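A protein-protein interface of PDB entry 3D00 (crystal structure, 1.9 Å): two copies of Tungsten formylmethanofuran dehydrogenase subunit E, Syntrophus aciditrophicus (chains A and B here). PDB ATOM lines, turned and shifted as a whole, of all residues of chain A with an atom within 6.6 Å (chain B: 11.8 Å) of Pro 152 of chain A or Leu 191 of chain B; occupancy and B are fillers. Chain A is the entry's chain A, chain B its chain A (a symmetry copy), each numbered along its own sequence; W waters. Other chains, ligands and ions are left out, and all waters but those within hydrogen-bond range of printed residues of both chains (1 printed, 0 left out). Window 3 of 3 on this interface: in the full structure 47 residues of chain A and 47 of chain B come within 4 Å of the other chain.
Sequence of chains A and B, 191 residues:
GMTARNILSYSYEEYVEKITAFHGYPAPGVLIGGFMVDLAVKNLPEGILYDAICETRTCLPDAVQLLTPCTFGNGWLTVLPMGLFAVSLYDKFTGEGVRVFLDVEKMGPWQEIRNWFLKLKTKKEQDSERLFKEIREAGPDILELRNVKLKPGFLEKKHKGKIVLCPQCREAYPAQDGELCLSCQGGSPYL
O of Ser 183 of chain B is in hydrogen-bond range of N of Ser 188 of chain B, 3.1 Å away.
The backbone NH (N) of Tyr 190 of chain B lies within hydrogen-bond range of the side-chain hydroxyl (OG) of Ser 188 of chain B (3.2 Å).
Among the printed residues, merely in contact across the chains: Lys 151 of chain A with Ser 188 of chain B, Lys 151 of chain A with Tyr 190 of chain B, Lys 149 of chain A with Tyr 190 of chain B, Leu 150 of chain A with Pro 189 of chain B, Phe 154 of chain A with Pro 189 of chain B, Leu 150 of chain A with Leu 191 of chain B, Val 148 of chain A with Tyr 190 of chain B, Pro 152 of chain A with Leu 191 of chain B, Leu 150 of chain A with Tyr 190 of chain B and Lys 151 of chain A with Leu 191 of chain B.
Printed residues of chain B that touch a printed residue of chain A: Ser 188, Pro 189, Tyr 190 and Leu 191.
Among the printed residues, 12 pairs touch across the chains.
No position is printed for both chains.
Of the 12 pairs that touch across the chains among the printed residues, none has its exchanged pair printed and touching as well.
Water W1 bridges the chain-end carboxylate of Leu 191 of chain B (2.7 Å) and the backbone NH of Lys 149 of chain A (3.0 Å).
Pro 152 of chain A touches one residue of chain B.
Val 148 of chain A touches just one residue of chain B: Tyr 190.
Of chain B, only Tyr 190 (3.3 Å) and Leu 191 (2.8 Å) come within 4 Å of Lys 149 of chain A.
Of chain B, only Pro 189 (3.5 Å), Tyr 190 (3.9 Å) and Leu 191 (3.7 Å) come within 4 Å of Leu 150 of chain A.
Lys 151 of chain A touches just these residues of chain B: Ser 188, Pro 189, Tyr 190 and Leu 191.
No residue of chain B comes within 4 Å of Gly 153 of chain A.
No residue of chain B comes within 4 Å of Glu 156 of chain A.
Printed residues of chain A within 4 Å of Tyr 190 of chain B: Val 148, Lys 149, Leu 150 and Lys 151.
Of the printed residues of chain A, Pro 189 of chain B touches Leu 150, Lys 151 and Phe 154.
Gly 186 of chain B touches none of the printed residues of chain A.
Gly 187 of chain B touches none of the printed residues of chain A.
The nearest residue of chain B that does not touch Pro 152 of chain A is Pro 189 of chain B (5.9 Å).
The nearest residue of chain A that does not touch Leu 191 of chain B is Val 148 of chain A (6.1 Å).
The nearest printed residue of chain A that does not touch Tyr 190 of chain B is Phe 154 of chain A (5.9 Å).
The backbone carbonyl oxygen of Lys 149 of chain A sits at hydrogen-bond distance from the backbone NH of Leu 191 of chain B (2.8 Å).
The backbone NH (N) of Lys 151 of chain A sits at hydrogen-bond distance from the backbone carbonyl oxygen (O) of Pro 189 of chain B, 2.7 Å away.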
ATOM      1  N   VAL A 148      17.517  28.503  18.689  1.00  0.00           N
ATOM      2  CA  VAL A 148      16.462  28.739  19.664  1.00  0.00           C
ATOM      3  C   VAL A 148      16.129  30.230  19.770  1.00  0.00           C
ATOM      4  O   VAL A 148      16.933  31.080  19.422  1.00  0.00           O
ATOM      5  CB  VAL A 148      16.839  28.160  21.074  1.00  0.00           C
ATOM      6  CG1 VAL A 148      17.022  26.648  21.013  1.00  0.00           C
ATOM      7  CG2 VAL A 148      18.079  28.865  21.696  1.00  0.00           C
ATOM      8  N   LYS A 149      14.937  30.534  20.259  1.00  0.00           N
ATOM      9  CA  LYS A 149      14.601  31.882  20.691  1.00  0.00           C
ATOM     10  C   LYS A 149      14.037  31.822  22.109  1.00  0.00           C
ATOM     11  O   LYS A 149      13.195  30.985  22.440  1.00  0.00           O
ATOM     12  CB  LYS A 149      13.609  32.511  19.749  1.00  0.00           C
ATOM     13  CG  LYS A 149      13.205  33.945  20.090  1.00  0.00           C
ATOM     14  N   LEU A 150      14.538  32.704  22.964  1.00  0.00           N
ATOM     15  CA  LEU A 150      14.143  32.702  24.356  1.00  0.00           C
ATOM     16  C   LEU A 150      12.690  33.185  24.517  1.00  0.00           C
ATOM     17  O   LEU A 150      12.185  33.984  23.726  1.00  0.00           O
ATOM     18  CB  LEU A 150      15.125  33.526  25.213  1.00  0.00           C
ATOM     19  CG  LEU A 150      16.421  32.797  25.581  1.00  0.00           C
ATOM     20  CD1 LEU A 150      16.189  31.728  26.658  1.00  0.00           C
ATOM     21  CD2 LEU A 150      17.138  32.145  24.356  1.00  0.00           C
ATOM     22  N   LYS A 151      12.034  32.638  25.539  1.00  0.00           N
ATOM     23  CA  LYS A 151      10.707  33.084  25.979  1.00  0.00           C
ATOM     24  C   LYS A 151      10.798  34.531  26.479  1.00  0.00           C
ATOM     25  O   LYS A 151      11.788  34.893  27.085  1.00  0.00           O
ATOM     26  CB  LYS A 151      10.165  32.157  27.094  1.00  0.00           C
ATOM     27  CG  LYS A 151       9.480  30.858  26.577  1.00  0.00           C
ATOM     28  CD  LYS A 151       9.118  29.878  27.701  1.00  0.00           C
ATOM     29  CE  LYS A 151       8.634  28.522  27.133  1.00  0.00           C
ATOM     30  N   PRO A 152       9.775  35.361  26.208  1.00  0.00           N
ATOM     31  CA  PRO A 152       9.702  36.739  26.742  1.00  0.00           C
ATOM     32  C   PRO A 152      10.199  36.982  28.189  1.00  0.00           C
ATOM     33  O   PRO A 152      10.928  37.933  28.415  1.00  0.00           O
ATOM     34  CB  PRO A 152       8.226  37.064  26.613  1.00  0.00           C
ATOM     35  CG  PRO A 152       7.808  36.348  25.363  1.00  0.00           C
ATOM     36  CD  PRO A 152       8.620  35.064  25.331  1.00  0.00           C
ATOM     37  N   GLY A 153       9.863  36.122  29.147  1.00  0.00           N
ATOM     38  CA  GLY A 153      10.245  36.335  30.543  1.00  0.00           C
ATOM     39  C   GLY A 153      11.739  36.397  30.797  1.00  0.00           C
ATOM     40  O   GLY A 153      12.187  36.956  31.817  1.00  0.00           O
ATOM     41  N   PHE A 154      12.526  35.842  29.880  1.00  0.00           N
ATOM     42  CA  PHE A 154      13.976  35.867  30.013  1.00  0.00           C
ATOM     43  C   PHE A 154      14.625  37.144  29.518  1.00  0.00           C
ATOM     44  O   PHE A 154      15.840  37.285  29.621  1.00  0.00           O
ATOM     45  CB  PHE A 154      14.594  34.643  29.318  1.00  0.00           C
ATOM     46  CG  PHE A 154      14.462  33.415  30.137  1.00  0.00           C
ATOM     47  CD1 PHE A 154      13.257  32.721  30.168  1.00  0.00           C
ATOM     48  CD2 PHE A 154      15.478  33.019  30.975  1.00  0.00           C
ATOM     49  CE1 PHE A 154      13.089  31.595  30.987  1.00  0.00           C
ATOM     50  CE2 PHE A 154      15.308  31.916  31.778  1.00  0.00           C
ATOM     51  CZ  PHE A 154      14.088  31.207  31.790  1.00  0.00           C
ATOM     52  N   LEU A 155      13.828  38.048  28.958  1.00  0.00           N
ATOM     53  CA  LEU A 155      14.315  39.300  28.414  1.00  0.00           C
ATOM     54  C   LEU A 155      13.481  40.428  29.038  1.00  0.00           C
ATOM     55  O   LEU A 155      13.206  41.448  28.399  1.00  0.00           O
ATOM     56  CB  LEU A 155      14.154  39.290  26.887  1.00  0.00           C
ATOM     57  CG  LEU A 155      14.708  38.125  26.050  1.00  0.00           C
ATOM     58  CD1 LEU A 155      14.137  38.189  24.643  1.00  0.00           C
ATOM     59  CD2 LEU A 155      16.228  38.160  26.006  1.00  0.00           C
ATOM     60  N   GLU A 156      13.039  40.239  30.276  1.00  0.00           N
ATOM     61  CA  GLU A 156      12.188  41.250  30.932  1.00  0.00           C
ATOM     62  C   GLU A 156      13.073  42.417  31.407  1.00  0.00           C
ATOM     63  O   GLU A 156      14.267  42.228  31.696  1.00  0.00           O
ATOM     64  CB  GLU A 156      11.402  40.634  32.113  1.00  0.00           C
ATOM     65  CG  GLU A 156      12.257  39.799  33.107  1.00  0.00           C
ATOM     66  N   GLN B 168      10.173  13.027  25.078  1.00  0.00           N
ATOM     67  CA  GLN B 168       9.744  14.146  24.286  1.00  0.00           C
ATOM     68  C   GLN B 168      10.903  14.822  23.555  1.00  0.00           C
ATOM     69  O   GLN B 168      10.796  15.092  22.347  1.00  0.00           O
ATOM     70  CB  GLN B 168       8.968  15.142  25.147  1.00  0.00           C
ATOM     71  CG  GLN B 168       8.221  16.137  24.318  1.00  0.00           C
ATOM     72  CD  GLN B 168       7.661  17.251  25.118  1.00  0.00           C
ATOM     73  OE1 GLN B 168       6.946  17.044  26.109  1.00  0.00           O
ATOM     74  NE2 GLN B 168       7.989  18.466  24.703  1.00  0.00           N
ATOM     75  N   CYS B 169      12.014  15.077  24.253  1.00  0.00           N
ATOM     76  CA  CYS B 169      13.156  15.748  23.619  1.00  0.00           C
ATOM     77  C   CYS B 169      14.337  14.838  23.356  1.00  0.00           C
ATOM     78  O   CYS B 169      15.280  15.255  22.684  1.00  0.00           O
ATOM     79  CB  CYS B 169      13.619  16.939  24.457  1.00  0.00           C
ATOM     80  SG  CYS B 169      14.498  16.487  25.959  1.00  0.00           S
ATOM     81  N   SER B 183      12.601  20.418  31.598  1.00  0.00           N
ATOM     82  CA  SER B 183      12.404  21.349  30.501  1.00  0.00           C
ATOM     83  C   SER B 183      11.073  21.051  29.822  1.00  0.00           C
ATOM     84  O   SER B 183      10.221  21.934  29.677  1.00  0.00           O
ATOM     85  CB  SER B 183      13.568  21.302  29.497  1.00  0.00           C
ATOM     86  OG  SER B 183      13.362  22.237  28.455  1.00  0.00           O
ATOM     87  N   CYS B 184      10.883  19.792  29.430  1.00  0.00           N
ATOM     88  CA  CYS B 184       9.665  19.365  28.744  1.00  0.00           C
ATOM     89  C   CYS B 184       8.423  19.453  29.633  1.00  0.00           C
ATOM     90  O   CYS B 184       7.290  19.601  29.137  1.00  0.00           O
ATOM     91  CB  CYS B 184       9.866  17.947  28.162  1.00  0.00           C
ATOM     92  SG  CYS B 184      10.886  17.975  26.679  1.00  0.00           S
ATOM     93  N   GLY B 186       7.941  21.979  31.424  1.00  0.00           N
ATOM     94  CA  GLY B 186       7.559  23.395  31.379  1.00  0.00           C
ATOM     95  C   GLY B 186       8.656  24.371  31.748  1.00  0.00           C
ATOM     96  O   GLY B 186       8.485  25.577  31.597  1.00  0.00           O
ATOM     97  N   GLY B 187       9.789  23.865  32.221  1.00  0.00           N
ATOM     98  CA  GLY B 187      10.903  24.717  32.558  1.00  0.00           C
ATOM     99  C   GLY B 187      11.645  25.290  31.356  1.00  0.00           C
ATOM    100  O   GLY B 187      12.494  26.152  31.536  1.00  0.00           O
ATOM    101  N   SER B 188      11.370  24.789  30.145  1.00  0.00           N
ATOM    102  CA  SER B 188      12.010  25.289  28.953  1.00  0.00           C
ATOM    103  C   SER B 188      11.970  26.807  28.895  1.00  0.00           C
ATOM    104  O   SER B 188      10.906  27.406  28.964  1.00  0.00           O
ATOM    105  CB  SER B 188      11.372  24.747  27.675  1.00  0.00           C
ATOM    106  OG  SER B 188      12.106  25.218  26.555  1.00  0.00           O
ATOM    107  N   PRO B 189      13.139  27.443  28.761  1.00  0.00           N
ATOM    108  CA  PRO B 189      13.191  28.855  28.478  1.00  0.00           C
ATOM    109  C   PRO B 189      12.953  29.247  27.009  1.00  0.00           C
ATOM    110  O   PRO B 189      12.962  30.436  26.714  1.00  0.00           O
ATOM    111  CB  PRO B 189      14.619  29.200  28.883  1.00  0.00           C
ATOM    112  CG  PRO B 189      15.368  28.006  28.588  1.00  0.00           C
ATOM    113  CD  PRO B 189      14.489  26.871  28.920  1.00  0.00           C
ATOM    114  N   TYR B 190      12.755  28.287  26.106  1.00  0.00           N
ATOM    115  CA  TYR B 190      12.788  28.571  24.676  1.00  0.00           C
ATOM    116  C   TYR B 190      11.392  28.499  24.146  1.00  0.00           C
ATOM    117  O   TYR B 190      10.549  27.795  24.702  1.00  0.00           O
ATOM    118  CB  TYR B 190      13.654  27.571  23.931  1.00  0.00           C
ATOM    119  CG  TYR B 190      14.990  27.329  24.596  1.00  0.00           C
ATOM    120  CD1 TYR B 190      15.911  28.345  24.694  1.00  0.00           C
ATOM    121  CD2 TYR B 190      15.308  26.103  25.139  1.00  0.00           C
ATOM    122  CE1 TYR B 190      17.164  28.147  25.354  1.00  0.00           C
ATOM    123  CE2 TYR B 190      16.560  25.893  25.789  1.00  0.00           C
ATOM    124  CZ  TYR B 190      17.474  26.935  25.885  1.00  0.00           C
ATOM    125  OH  TYR B 190      18.726  26.793  26.525  1.00  0.00           O
ATOM    126  N   LEU B 191      11.154  29.232  23.068  1.00  0.00           N
ATOM    127  CA  LEU B 191       9.850  29.249  22.421  1.00  0.00           C
ATOM    128  C   LEU B 191       9.634  27.970  21.628  1.00  0.00           C
ATOM    129  O   LEU B 191      10.579  27.299  21.172  1.00  0.00           O
ATOM    130  CB  LEU B 191       9.713  30.431  21.462  1.00  0.00           C
ATOM    131  CG  LEU B 191       9.664  31.853  22.012  1.00  0.00           C
ATOM    132  CD1 LEU B 191       9.701  32.797  20.820  1.00  0.00           C
ATOM    133  CD2 LEU B 191       8.445  32.102  22.898  1.00  0.00           C
ATOM    134  OXT LEU B 191       8.459  27.616  21.399  1.00  0.00           O
HETATM  135  O   HOH W   1      13.009  28.221  20.415  1.00  0.00           O
